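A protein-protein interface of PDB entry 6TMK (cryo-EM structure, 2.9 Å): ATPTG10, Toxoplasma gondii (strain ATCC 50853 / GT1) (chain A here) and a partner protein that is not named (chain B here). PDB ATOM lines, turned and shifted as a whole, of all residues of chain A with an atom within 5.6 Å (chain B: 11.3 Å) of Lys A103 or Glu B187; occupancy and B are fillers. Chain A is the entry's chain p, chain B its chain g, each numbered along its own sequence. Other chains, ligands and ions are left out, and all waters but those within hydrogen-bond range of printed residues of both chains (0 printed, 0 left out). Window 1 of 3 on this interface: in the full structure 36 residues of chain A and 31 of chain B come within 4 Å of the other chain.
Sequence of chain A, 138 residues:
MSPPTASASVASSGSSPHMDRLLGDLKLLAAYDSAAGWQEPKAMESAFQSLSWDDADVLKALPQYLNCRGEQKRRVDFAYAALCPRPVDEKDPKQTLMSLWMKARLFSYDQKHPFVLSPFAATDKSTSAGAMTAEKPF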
ATOM      1  N   TYR A  65     -19.062   7.473 -22.983  1.00  0.00           N
ATOM      2  CA  TYR A  65     -19.053   7.328 -24.432  1.00  0.00           C
ATOM      3  C   TYR A  65     -18.367   6.038 -24.842  1.00  0.00           C
ATOM      4  O   TYR A  65     -18.801   5.364 -25.783  1.00  0.00           O
ATOM      5  CB  TYR A  65     -18.355   8.515 -25.088  1.00  0.00           C
ATOM      6  CG  TYR A  65     -18.072   8.265 -26.545  1.00  0.00           C
ATOM      7  CD1 TYR A  65     -19.096   8.254 -27.477  1.00  0.00           C
ATOM      8  CD2 TYR A  65     -16.787   8.006 -26.986  1.00  0.00           C
ATOM      9  CE1 TYR A  65     -18.846   8.010 -28.803  1.00  0.00           C
ATOM     10  CE2 TYR A  65     -16.528   7.758 -28.311  1.00  0.00           C
ATOM     11  CZ  TYR A  65     -17.562   7.762 -29.216  1.00  0.00           C
ATOM     12  OH  TYR A  65     -17.320   7.514 -30.543  1.00  0.00           O
ATOM     13  N   LEU A  66     -17.289   5.677 -24.149  1.00  0.00           N
ATOM     14  CA  LEU A  66     -16.536   4.491 -24.531  1.00  0.00           C
ATOM     15  C   LEU A  66     -17.343   3.213 -24.359  1.00  0.00           C
ATOM     16  O   LEU A  66     -16.966   2.180 -24.920  1.00  0.00           O
ATOM     17  CB  LEU A  66     -15.256   4.396 -23.709  1.00  0.00           C
ATOM     18  CG  LEU A  66     -14.157   5.403 -24.032  1.00  0.00           C
ATOM     19  CD1 LEU A  66     -13.070   5.346 -22.987  1.00  0.00           C
ATOM     20  CD2 LEU A  66     -13.579   5.128 -25.396  1.00  0.00           C
ATOM     21  N   VAL A  76     -24.071  10.497 -32.035  1.00  0.00           N
ATOM     22  CA  VAL A  76     -22.796  11.160 -31.802  1.00  0.00           C
ATOM     23  C   VAL A  76     -21.832  10.899 -32.951  1.00  0.00           C
ATOM     24  O   VAL A  76     -21.068  11.785 -33.350  1.00  0.00           O
ATOM     25  CB  VAL A  76     -22.213  10.707 -30.455  1.00  0.00           C
ATOM     26  CG1 VAL A  76     -20.822  11.255 -30.269  1.00  0.00           C
ATOM     27  CG2 VAL A  76     -23.116  11.149 -29.339  1.00  0.00           C
ATOM     28  N   ASP A  77     -21.856   9.690 -33.508  1.00  0.00           N
ATOM     29  CA  ASP A  77     -21.018   9.383 -34.660  1.00  0.00           C
ATOM     30  C   ASP A  77     -21.413  10.218 -35.869  1.00  0.00           C
ATOM     31  O   ASP A  77     -20.551  10.689 -36.614  1.00  0.00           O
ATOM     32  CB  ASP A  77     -21.108   7.894 -34.976  1.00  0.00           C
ATOM     33  CG  ASP A  77     -20.317   7.046 -34.003  1.00  0.00           C
ATOM     34  OD1 ASP A  77     -20.069   5.862 -34.309  1.00  0.00           O
ATOM     35  OD2 ASP A  77     -19.939   7.565 -32.933  1.00  0.00           O
ATOM     36  N   TYR A  80     -20.105  13.720 -35.267  1.00  0.00           N
ATOM     37  CA  TYR A  80     -18.660  13.775 -35.406  1.00  0.00           C
ATOM     38  C   TYR A  80     -18.232  13.630 -36.855  1.00  0.00           C
ATOM     39  O   TYR A  80     -17.235  14.226 -37.259  1.00  0.00           O
ATOM     40  CB  TYR A  80     -17.999  12.702 -34.549  1.00  0.00           C
ATOM     41  CG  TYR A  80     -16.500  12.711 -34.669  1.00  0.00           C
ATOM     42  CD1 TYR A  80     -15.745  13.660 -34.009  1.00  0.00           C
ATOM     43  CD2 TYR A  80     -15.840  11.783 -35.452  1.00  0.00           C
ATOM     44  CE1 TYR A  80     -14.383  13.681 -34.119  1.00  0.00           C
ATOM     45  CE2 TYR A  80     -14.478  11.798 -35.567  1.00  0.00           C
ATOM     46  CZ  TYR A  80     -13.753  12.746 -34.899  1.00  0.00           C
ATOM     47  OH  TYR A  80     -12.387  12.758 -35.017  1.00  0.00           O
ATOM     48  N   THR A  96      -5.886  10.511 -32.370  1.00  0.00           N
ATOM     49  CA  THR A  96      -6.874   9.645 -31.736  1.00  0.00           C
ATOM     50  C   THR A  96      -7.464  10.300 -30.494  1.00  0.00           C
ATOM     51  O   THR A  96      -8.679  10.252 -30.267  1.00  0.00           O
ATOM     52  CB  THR A  96      -6.232   8.306 -31.385  1.00  0.00           C
ATOM     53  OG1 THR A  96      -5.846   7.632 -32.587  1.00  0.00           O
ATOM     54  CG2 THR A  96      -7.200   7.440 -30.617  1.00  0.00           C
ATOM     55  N   MET A  98      -7.562  13.573 -29.606  1.00  0.00           N
ATOM     56  CA  MET A  98      -8.400  14.731 -29.893  1.00  0.00           C
ATOM     57  C   MET A  98      -9.758  14.297 -30.426  1.00  0.00           C
ATOM     58  O   MET A  98     -10.790  14.893 -30.084  1.00  0.00           O
ATOM     59  CB  MET A  98      -7.694  15.653 -30.875  1.00  0.00           C
ATOM     60  CG  MET A  98      -6.480  16.315 -30.285  1.00  0.00           C
ATOM     61  SD  MET A  98      -5.916  17.740 -31.219  1.00  0.00           S
ATOM     62  CE  MET A  98      -5.252  16.911 -32.647  1.00  0.00           C
ATOM     63  N   SER A  99      -9.783  13.256 -31.256  1.00  0.00           N
ATOM     64  CA  SER A  99     -11.053  12.699 -31.704  1.00  0.00           C
ATOM     65  C   SER A  99     -11.887  12.224 -30.522  1.00  0.00           C
ATOM     66  O   SER A  99     -13.087  12.512 -30.434  1.00  0.00           O
ATOM     67  CB  SER A  99     -10.799  11.559 -32.683  1.00  0.00           C
ATOM     68  OG  SER A  99      -9.909  11.966 -33.703  1.00  0.00           O
ATOM     69  N   LEU A 100     -11.266  11.476 -29.610  1.00  0.00           N
ATOM     70  CA  LEU A 100     -11.978  10.997 -28.431  1.00  0.00           C
ATOM     71  C   LEU A 100     -12.527  12.153 -27.609  1.00  0.00           C
ATOM     72  O   LEU A 100     -13.651  12.089 -27.102  1.00  0.00           O
ATOM     73  CB  LEU A 100     -11.055  10.138 -27.577  1.00  0.00           C
ATOM     74  CG  LEU A 100     -10.878   8.700 -28.038  1.00  0.00           C
ATOM     75  CD1 LEU A 100      -9.652   8.108 -27.402  1.00  0.00           C
ATOM     76  CD2 LEU A 100     -12.099   7.889 -27.692  1.00  0.00           C
ATOM     77  N   TRP A 101     -11.740  13.215 -27.458  1.00  0.00           N
ATOM     78  CA  TRP A 101     -12.165  14.352 -26.655  1.00  0.00           C
ATOM     79  C   TRP A 101     -13.371  15.037 -27.281  1.00  0.00           C
ATOM     80  O   TRP A 101     -14.349  15.365 -26.594  1.00  0.00           O
ATOM     81  CB  TRP A 101     -11.006  15.333 -26.512  1.00  0.00           C
ATOM     82  CG  TRP A 101     -11.170  16.294 -25.397  1.00  0.00           C
ATOM     83  CD1 TRP A 101     -11.263  17.643 -25.489  1.00  0.00           C
ATOM     84  CD2 TRP A 101     -11.254  15.979 -24.006  1.00  0.00           C
ATOM     85  NE1 TRP A 101     -11.404  18.194 -24.244  1.00  0.00           N
ATOM     86  CE2 TRP A 101     -11.401  17.190 -23.315  1.00  0.00           C
ATOM     87  CE3 TRP A 101     -11.223  14.789 -23.279  1.00  0.00           C
ATOM     88  CZ2 TRP A 101     -11.516  17.248 -21.936  1.00  0.00           C
ATOM     89  CZ3 TRP A 101     -11.336  14.849 -21.914  1.00  0.00           C
ATOM     90  CH2 TRP A 101     -11.481  16.068 -21.255  1.00  0.00           C
ATOM     91  N   MET A 102     -13.320  15.260 -28.594  1.00  0.00           N
ATOM     92  CA  MET A 102     -14.446  15.885 -29.277  1.00  0.00           C
ATOM     93  C   MET A 102     -15.694  15.017 -29.179  1.00  0.00           C
ATOM     94  O   MET A 102     -16.801  15.524 -28.946  1.00  0.00           O
ATOM     95  CB  MET A 102     -14.074  16.148 -30.734  1.00  0.00           C
ATOM     96  CG  MET A 102     -15.204  16.662 -31.594  1.00  0.00           C
ATOM     97  SD  MET A 102     -16.200  17.945 -30.813  1.00  0.00           S
ATOM     98  CE  MET A 102     -15.006  19.269 -30.699  1.00  0.00           C
ATOM     99  N   LYS A 103     -15.532  13.704 -29.336  1.00  0.00           N
ATOM    100  CA  LYS A 103     -16.671  12.804 -29.231  1.00  0.00           C
ATOM    101  C   LYS A 103     -17.257  12.812 -27.828  1.00  0.00           C
ATOM    102  O   LYS A 103     -18.478  12.758 -27.661  1.00  0.00           O
ATOM    103  CB  LYS A 103     -16.256  11.397 -29.633  1.00  0.00           C
ATOM    104  CG  LYS A 103     -16.040  11.244 -31.108  1.00  0.00           C
ATOM    105  CD  LYS A 103     -15.902   9.806 -31.511  1.00  0.00           C
ATOM    106  CE  LYS A 103     -14.874   9.636 -32.594  1.00  0.00           C
ATOM    107  NZ  LYS A 103     -15.147   8.447 -33.432  1.00  0.00           N
ATOM    108  N   ALA A 104     -16.406  12.873 -26.805  1.00  0.00           N
ATOM    109  CA  ALA A 104     -16.900  12.927 -25.436  1.00  0.00           C
ATOM    110  C   ALA A 104     -17.658  14.219 -25.175  1.00  0.00           C
ATOM    111  O   ALA A 104     -18.680  14.221 -24.480  1.00  0.00           O
ATOM    112  CB  ALA A 104     -15.736  12.787 -24.468  1.00  0.00           C
ATOM    113  N   ARG A 105     -17.168  15.329 -25.722  1.00  0.00           N
ATOM    114  CA  ARG A 105     -17.875  16.596 -25.589  1.00  0.00           C
ATOM    115  C   ARG A 105     -19.263  16.510 -26.212  1.00  0.00           C
ATOM    116  O   ARG A 105     -20.267  16.914 -25.604  1.00  0.00           O
ATOM    117  CB  ARG A 105     -17.058  17.701 -26.247  1.00  0.00           C
ATOM    118  CG  ARG A 105     -17.688  19.061 -26.185  1.00  0.00           C
ATOM    119  CD  ARG A 105     -16.727  20.128 -26.653  1.00  0.00           C
ATOM    120  NE  ARG A 105     -15.606  20.311 -25.742  1.00  0.00           N
ATOM    121  CZ  ARG A 105     -15.684  20.947 -24.580  1.00  0.00           C
ATOM    122  NH1 ARG A 105     -16.830  21.473 -24.180  1.00  0.00           N
ATOM    123  NH2 ARG A 105     -14.612  21.063 -23.817  1.00  0.00           N
ATOM    124  N   LEU A 106     -19.336  15.975 -27.430  1.00  0.00           N
ATOM    125  CA  LEU A 106     -20.627  15.830 -28.089  1.00  0.00           C
ATOM    126  C   LEU A 106     -21.533  14.873 -27.326  1.00  0.00           C
ATOM    127  O   LEU A 106     -22.747  15.080 -27.261  1.00  0.00           O
ATOM    128  CB  LEU A 106     -20.425  15.345 -29.518  1.00  0.00           C
ATOM    129  CG  LEU A 106     -19.579  16.244 -30.408  1.00  0.00           C
ATOM    130  CD1 LEU A 106     -19.264  15.524 -31.690  1.00  0.00           C
ATOM    131  CD2 LEU A 106     -20.268  17.553 -30.687  1.00  0.00           C
ATOM    132  N   PHE A 107     -20.960  13.824 -26.736  1.00  0.00           N
ATOM    133  CA  PHE A 107     -21.753  12.892 -25.945  1.00  0.00           C
ATOM    134  C   PHE A 107     -22.352  13.582 -24.731  1.00  0.00           C
ATOM    135  O   PHE A 107     -23.512  13.342 -24.377  1.00  0.00           O
ATOM    136  CB  PHE A 107     -20.888  11.710 -25.522  1.00  0.00           C
ATOM    137  CG  PHE A 107     -21.636  10.642 -24.789  1.00  0.00           C
ATOM    138  CD1 PHE A 107     -22.271   9.628 -25.477  1.00  0.00           C
ATOM    139  CD2 PHE A 107     -21.703  10.650 -23.412  1.00  0.00           C
ATOM    140  CE1 PHE A 107     -22.960   8.649 -24.805  1.00  0.00           C
ATOM    141  CE2 PHE A 107     -22.390   9.674 -22.738  1.00  0.00           C
ATOM    142  CZ  PHE A 107     -23.019   8.672 -23.435  1.00  0.00           C
ATOM    143  N   SER A 108     -21.569  14.430 -24.069  1.00  0.00           N
ATOM    144  CA  SER A 108     -22.082  15.167 -22.922  1.00  0.00           C
ATOM    145  C   SER A 108     -23.235  16.068 -23.342  1.00  0.00           C
ATOM    146  O   SER A 108     -24.303  16.079 -22.709  1.00  0.00           O
ATOM    147  CB  SER A 108     -20.961  15.981 -22.285  1.00  0.00           C
ATOM    148  OG  SER A 108     -20.575  17.051 -23.118  1.00  0.00           O
ATOM    149  N   VAL B 180     -21.727   5.888 -42.223  1.00  0.00           N
ATOM    150  CA  VAL B 180     -20.814   7.015 -42.099  1.00  0.00           C
ATOM    151  C   VAL B 180     -19.404   6.459 -42.028  1.00  0.00           C
ATOM    152  O   VAL B 180     -19.199   5.244 -42.127  1.00  0.00           O
ATOM    153  CB  VAL B 180     -21.128   7.893 -40.876  1.00  0.00           C
ATOM    154  CG1 VAL B 180     -22.538   8.427 -40.954  1.00  0.00           C
ATOM    155  CG2 VAL B 180     -20.917   7.122 -39.598  1.00  0.00           C
ATOM    156  N   THR B 181     -18.430   7.336 -41.857  1.00  0.00           N
ATOM    157  CA  THR B 181     -17.052   6.891 -41.798  1.00  0.00           C
ATOM    158  C   THR B 181     -16.880   5.934 -40.621  1.00  0.00           C
ATOM    159  O   THR B 181     -17.401   6.194 -39.531  1.00  0.00           O
ATOM    160  CB  THR B 181     -16.112   8.082 -41.655  1.00  0.00           C
ATOM    161  OG1 THR B 181     -16.436   9.068 -42.641  1.00  0.00           O
ATOM    162  CG2 THR B 181     -14.682   7.649 -41.829  1.00  0.00           C
ATOM    163  N   PRO B 182     -16.167   4.825 -40.797  1.00  0.00           N
ATOM    164  CA  PRO B 182     -16.028   3.869 -39.698  1.00  0.00           C
ATOM    165  C   PRO B 182     -15.256   4.452 -38.530  1.00  0.00           C
ATOM    166  O   PRO B 182     -14.515   5.430 -38.651  1.00  0.00           O
ATOM    167  CB  PRO B 182     -15.265   2.701 -40.333  1.00  0.00           C
ATOM    168  CG  PRO B 182     -15.414   2.882 -41.787  1.00  0.00           C
ATOM    169  CD  PRO B 182     -15.504   4.340 -42.016  1.00  0.00           C
ATOM    170  N   GLU B 183     -15.441   3.817 -37.379  1.00  0.00           N
ATOM    171  CA  GLU B 183     -14.794   4.252 -36.155  1.00  0.00           C
ATOM    172  C   GLU B 183     -13.352   3.768 -36.095  1.00  0.00           C
ATOM    173  O   GLU B 183     -12.999   2.718 -36.639  1.00  0.00           O
ATOM    174  CB  GLU B 183     -15.565   3.740 -34.940  1.00  0.00           C
ATOM    175  CG  GLU B 183     -15.186   4.411 -33.635  1.00  0.00           C
ATOM    176  CD  GLU B 183     -15.923   3.833 -32.447  1.00  0.00           C
ATOM    177  OE1 GLU B 183     -16.913   3.101 -32.658  1.00  0.00           O
ATOM    178  OE2 GLU B 183     -15.514   4.108 -31.301  1.00  0.00           O
ATOM    179  N   ASN B 184     -12.525   4.549 -35.425  1.00  0.00           N
ATOM    180  CA  ASN B 184     -11.140   4.172 -35.210  1.00  0.00           C
ATOM    181  C   ASN B 184     -11.076   2.936 -34.320  1.00  0.00           C
ATOM    182  O   ASN B 184     -11.665   2.935 -33.232  1.00  0.00           O
ATOM    183  CB  ASN B 184     -10.378   5.326 -34.576  1.00  0.00           C
ATOM    184  CG  ASN B 184      -8.891   5.218 -34.774  1.00  0.00           C
ATOM    185  OD1 ASN B 184      -8.355   4.131 -34.977  1.00  0.00           O
ATOM    186  ND2 ASN B 184      -8.210   6.350 -34.717  1.00  0.00           N
ATOM    187  N   PRO B 185     -10.387   1.869 -34.735  1.00  0.00           N
ATOM    188  CA  PRO B 185     -10.258   0.700 -33.850  1.00  0.00           C
ATOM    189  C   PRO B 185      -9.407   0.968 -32.627  1.00  0.00           C
ATOM    190  O   PRO B 185      -9.479   0.202 -31.654  1.00  0.00           O
ATOM    191  CB  PRO B 185      -9.608  -0.352 -34.755  1.00  0.00           C
ATOM    192  CG  PRO B 185      -8.918   0.443 -35.808  1.00  0.00           C
ATOM    193  CD  PRO B 185      -9.773   1.625 -36.047  1.00  0.00           C
ATOM    194  N   ALA B 186      -8.594   2.024 -32.652  1.00  0.00           N
ATOM    195  CA  ALA B 186      -7.792   2.365 -31.489  1.00  0.00           C
ATOM    196  C   ALA B 186      -8.670   2.715 -30.300  1.00  0.00           C
ATOM    197  O   ALA B 186      -8.270   2.507 -29.152  1.00  0.00           O
ATOM    198  CB  ALA B 186      -6.861   3.524 -31.825  1.00  0.00           C
ATOM    199  N   GLU B 187      -9.871   3.234 -30.549  1.00  0.00           N
ATOM    200  CA  GLU B 187     -10.748   3.614 -29.452  1.00  0.00           C
ATOM    201  C   GLU B 187     -11.247   2.408 -28.672  1.00  0.00           C
ATOM    202  O   GLU B 187     -11.639   2.558 -27.509  1.00  0.00           O
ATOM    203  CB  GLU B 187     -11.928   4.416 -29.990  1.00  0.00           C
ATOM    204  CG  GLU B 187     -11.523   5.737 -30.604  1.00  0.00           C
ATOM    205  CD  GLU B 187     -12.705   6.545 -31.096  1.00  0.00           C
ATOM    206  OE1 GLU B 187     -12.487   7.651 -31.633  1.00  0.00           O
ATOM    207  OE2 GLU B 187     -13.853   6.076 -30.944  1.00  0.00           O
ATOM    208  N   LYS B 188     -11.243   1.223 -29.277  1.00  0.00           N
ATOM    209  CA  LYS B 188     -11.621   0.000 -28.584  1.00  0.00           C
ATOM    210  C   LYS B 188     -10.429  -0.841 -28.159  1.00  0.00           C
ATOM    211  O   LYS B 188     -10.541  -1.607 -27.198  1.00  0.00           O
ATOM    212  CB  LYS B 188     -12.543  -0.854 -29.460  1.00  0.00           C
ATOM    213  CG  LYS B 188     -13.832  -0.165 -29.872  1.00  0.00           C
ATOM    214  CD  LYS B 188     -14.641   0.269 -28.659  1.00  0.00           C
ATOM    215  CE  LYS B 188     -16.019   0.770 -29.045  1.00  0.00           C
ATOM    216  NZ  LYS B 188     -16.958  -0.348 -29.337  1.00  0.00           N
ATOM    217  N   LEU B 189      -9.297  -0.721 -28.848  1.00  0.00           N
ATOM    218  CA  LEU B 189      -8.128  -1.521 -28.503  1.00  0.00           C
ATOM    219  C   LEU B 189      -7.228  -0.848 -27.473  1.00  0.00           C
ATOM    220  O   LEU B 189      -6.731  -1.514 -26.560  1.00  0.00           O
ATOM    221  CB  LEU B 189      -7.324  -1.838 -29.760  1.00  0.00           C
ATOM    222  CG  LEU B 189      -8.048  -2.703 -30.788  1.00  0.00           C
ATOM    223  CD1 LEU B 189      -7.223  -2.824 -32.041  1.00  0.00           C
ATOM    224  CD2 LEU B 189      -8.360  -4.076 -30.231  1.00  0.00           C
ATOM    225  N   LEU B 190      -7.011   0.457 -27.601  1.00  0.00           N
ATOM    226  CA  LEU B 190      -6.137   1.231 -26.722  1.00  0.00           C
ATOM    227  C   LEU B 190      -6.938   2.053 -25.725  1.00  0.00           C
ATOM    228  O   LEU B 190      -6.599   3.197 -25.417  1.00  0.00           O
ATOM    229  CB  LEU B 190      -5.227   2.127 -27.550  1.00  0.00           C
ATOM    230  CG  LEU B 190      -4.069   1.437 -28.265  1.00  0.00           C
ATOM    231  CD1 LEU B 190      -4.567   0.430 -29.270  1.00  0.00           C
ATOM    232  CD2 LEU B 190      -3.212   2.465 -28.951  1.00  0.00           C
ATOM    233  N   LYS B 191      -8.021   1.474 -25.211  1.00  0.00           N
ATOM    234  CA  LYS B 191      -8.954   2.213 -24.372  1.00  0.00           C
ATOM    235  C   LYS B 191      -8.277   2.697 -23.094  1.00  0.00           C
ATOM    236  O   LYS B 191      -8.276   3.897 -22.789  1.00  0.00           O
ATOM    237  CB  LYS B 191     -10.150   1.318 -24.055  1.00  0.00           C
ATOM    238  CG  LYS B 191     -11.282   1.996 -23.333  1.00  0.00           C
ATOM    239  CD  LYS B 191     -12.619   1.405 -23.746  1.00  0.00           C
ATOM    240  CE  LYS B 191     -12.712  -0.075 -23.417  1.00  0.00           C
ATOM    241  NZ  LYS B 191     -12.445  -0.355 -21.980  1.00  0.00           N
ATOM    242  N   GLU B 192      -7.689   1.773 -22.334  1.00  0.00           N
ATOM    243  CA  GLU B 192      -7.124   2.135 -21.040  1.00  0.00           C
ATOM    244  C   GLU B 192      -5.947   3.086 -21.201  1.00  0.00           C
ATOM    245  O   GLU B 192      -5.795   4.039 -20.425  1.00  0.00           O
ATOM    246  CB  GLU B 192      -6.693   0.878 -20.290  1.00  0.00           C
ATOM    247  CG  GLU B 192      -7.742  -0.226 -20.257  1.00  0.00           C
ATOM    248  CD  GLU B 192      -9.074   0.243 -19.703  1.00  0.00           C
ATOM    249  OE1 GLU B 192     -10.116  -0.051 -20.325  1.00  0.00           O
ATOM    250  OE2 GLU B 192      -9.080   0.908 -18.645  1.00  0.00           O
ATOM    251  N   GLU B 193      -5.103   2.845 -22.205  1.00  0.00           N
ATOM    252  CA  GLU B 193      -3.965   3.726 -22.443  1.00  0.00           C
ATOM    253  C   GLU B 193      -4.431   5.136 -22.767  1.00  0.00           C
ATOM    254  O   GLU B 193      -3.852   6.117 -22.287  1.00  0.00           O
ATOM    255  CB  GLU B 193      -3.112   3.173 -23.579  1.00  0.00           C
ATOM    256  CG  GLU B 193      -2.469   1.839 -23.277  1.00  0.00           C
ATOM    257  CD  GLU B 193      -3.362   0.667 -23.631  1.00  0.00           C
ATOM    258  OE1 GLU B 193      -2.896  -0.246 -24.340  1.00  0.00           O
ATOM    259  OE2 GLU B 193      -4.534   0.658 -23.196  1.00  0.00           O
ATOM    260  N   ALA B 194      -5.485   5.256 -23.574  1.00  0.00           N
ATOM    261  CA  ALA B 194      -5.989   6.572 -23.938  1.00  0.00           C
ATOM    262  C   ALA B 194      -6.601   7.274 -22.736  1.00  0.00           C
ATOM    263  O   ALA B 194      -6.420   8.484 -22.556  1.00  0.00           O
ATOM    264  CB  ALA B 194      -7.011   6.447 -25.063  1.00  0.00           C
ATOM    265  N   VAL B 195      -7.320   6.532 -21.894  1.00  0.00           N
ATOM    266  CA  VAL B 195      -7.901   7.142 -20.705  1.00  0.00           C
ATOM    267  C   VAL B 195      -6.801   7.639 -19.779  1.00  0.00           C
ATOM    268  O   VAL B 195      -6.899   8.728 -19.198  1.00  0.00           O
ATOM    269  CB  VAL B 195      -8.829   6.142 -19.996  1.00  0.00           C
ATOM    270  CG1 VAL B 195      -9.279   6.693 -18.661  1.00  0.00           C
ATOM    271  CG2 VAL B 195     -10.021   5.824 -20.867  1.00  0.00           C
ATOM    272  N   ALA B 196      -5.729   6.858 -19.636  1.00  0.00           N
ATOM    273  CA  ALA B 196      -4.623   7.284 -18.789  1.00  0.00           C
ATOM    274  C   ALA B 196      -3.921   8.505 -19.363  1.00  0.00           C
ATOM    275  O   ALA B 196      -3.547   9.420 -18.620  1.00  0.00           O
ATOM    276  CB  ALA B 196      -3.637   6.135 -18.615  1.00  0.00           C
ATOM    277  N   ILE B 198      -5.305  10.802 -21.183  1.00  0.00           N
ATOM    278  CA  ILE B 198      -6.178  11.955 -21.004  1.00  0.00           C
ATOM    279  C   ILE B 198      -6.168  12.413 -19.553  1.00  0.00           C
ATOM    280  O   ILE B 198      -6.239  13.613 -19.267  1.00  0.00           O
ATOM    281  CB  ILE B 198      -7.596  11.628 -21.498  1.00  0.00           C
ATOM    282  CG1 ILE B 198      -7.586  11.556 -23.025  1.00  0.00           C
ATOM    283  CG2 ILE B 198      -8.582  12.654 -20.981  1.00  0.00           C
ATOM    284  CD1 ILE B 198      -8.885  11.155 -23.654  1.00  0.00           C
ATOM    285  N   MET B 219       1.625   4.130 -26.178  1.00  0.00           N
ATOM    286  CA  MET B 219       0.626   4.015 -27.237  1.00  0.00           C
ATOM    287  C   MET B 219       1.280   3.915 -28.608  1.00  0.00           C
ATOM    288  O   MET B 219       0.886   3.088 -29.439  1.00  0.00           O
ATOM    289  CB  MET B 219      -0.305   5.219 -27.193  1.00  0.00           C
ATOM    290  CG  MET B 219      -1.148   5.313 -25.951  1.00  0.00           C
ATOM    291  SD  MET B 219      -1.896   6.938 -25.789  1.00  0.00           S
ATOM    292  CE  MET B 219      -3.187   6.808 -27.011  1.00  0.00           C
ATOM    293  N   ALA B 223       1.034   0.736 -31.200  1.00  0.00           N
ATOM    294  CA  ALA B 223       0.388   0.861 -32.499  1.00  0.00           C
ATOM    295  C   ALA B 223       1.340   0.583 -33.651  1.00  0.00           C
ATOM    296  O   ALA B 223       0.915   0.056 -34.683  1.00  0.00           O
ATOM    297  CB  ALA B 223      -0.210   2.256 -32.653  1.00  0.00           C
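The side-chain hydroxyl (OG1) of Thr A96 is in hydrogen-bond range of the side-chain amide nitrogen (ND2) of Asn B184 (3.4 Å).
OE1 of Glu B187 is in salt-bridge range of NZ of Lys A103, 3.3 Å away.
The side-chain carboxylate (OE2) of Glu B183 lies close to the side-chain carboxylate (OE2) of Glu B187, 2.6 Å away.
N of Ala B186 sits close to OD1 of Asn B184, at 3.1 Å.
The side-chain amino group (NZ) of Lys B191 is in salt-bridge range of the side-chain carboxylate (OE1) of Glu B192, at 2.9 Å.
Among the printed residues, pairs that only touch across the chains: Trp A101 with Ile B198, Leu A100 with Glu B187, Leu A66 with Val B195, Tyr A65 with Glu B187, Leu A66 with Lys B191, Leu A66 with Glu B187, Leu A100 with Ala B194 and Tyr A65 with Glu B183.
Of the printed residues of chain B, Tyr A65 touches Glu B183 and Glu B187.
Printed residues of chain B within 4 Å of Leu A66: Glu B187, Lys B191 and Val B195.
No residue of chain B comes within 4 Å of Asp A77.
No residue of chain B comes within 4 Å of Tyr A80.
Ser A99 touches none of the printed residues of chain B.
Of chain B, only Glu B187 (3.7 Å) and Ala B194 (3.9 Å) come within 4 Å of Leu A100.
No residue of chain B comes within 4 Å of Met A102.
Lys A103 touches just one residue of chain B: Glu B187 (3.2 Å).
No residue of chain B comes within 4 Å of Ala A104.
Glu B187 touches just these residues of chain A: Tyr A65 (3.8 Å), Leu A66 (3.9 Å), Leu A100 (3.7 Å) and Lys A103 (3.2 Å).
Leu B190 touches none of the printed residues of chain A.
Of the printed residues of chain A, Ala B194 touches Leu A100.
Printed residues of chain A within 4 Å of Val B195: Leu A66.
Printed residues of chain A within 4 Å of Ile B198: Trp A101 (3.6 Å).
The nearest residue of chain B that does not touch Lys A103 is Glu B183 (4.04 Å).
The nearest residue of chain A that does not touch Glu B187 is Ser A99 (4.4 Å).
The nearest printed residue of chain A that does not touch Lys B191 is Leu A100 (6.4 Å).
Of the 20 printed residues of chain B, 7 touch a printed residue of chain A.
Printed residues of chain B that touch a printed residue of chain A: Glu B183, Asn B184, Glu B187, Lys B191, Ala B194, Val B195 and Ile B198.
Of the 17 printed residues of chain A, 6 touch a printed residue of chain B.
Among the printed residues, 10 pairs touch across the chains.
Among the printed residues, Asp or Glu carboxylates within 4 Å of a Lys or Arg side-chain nitrogen of the other chain: Lys A103 with Glu B187.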
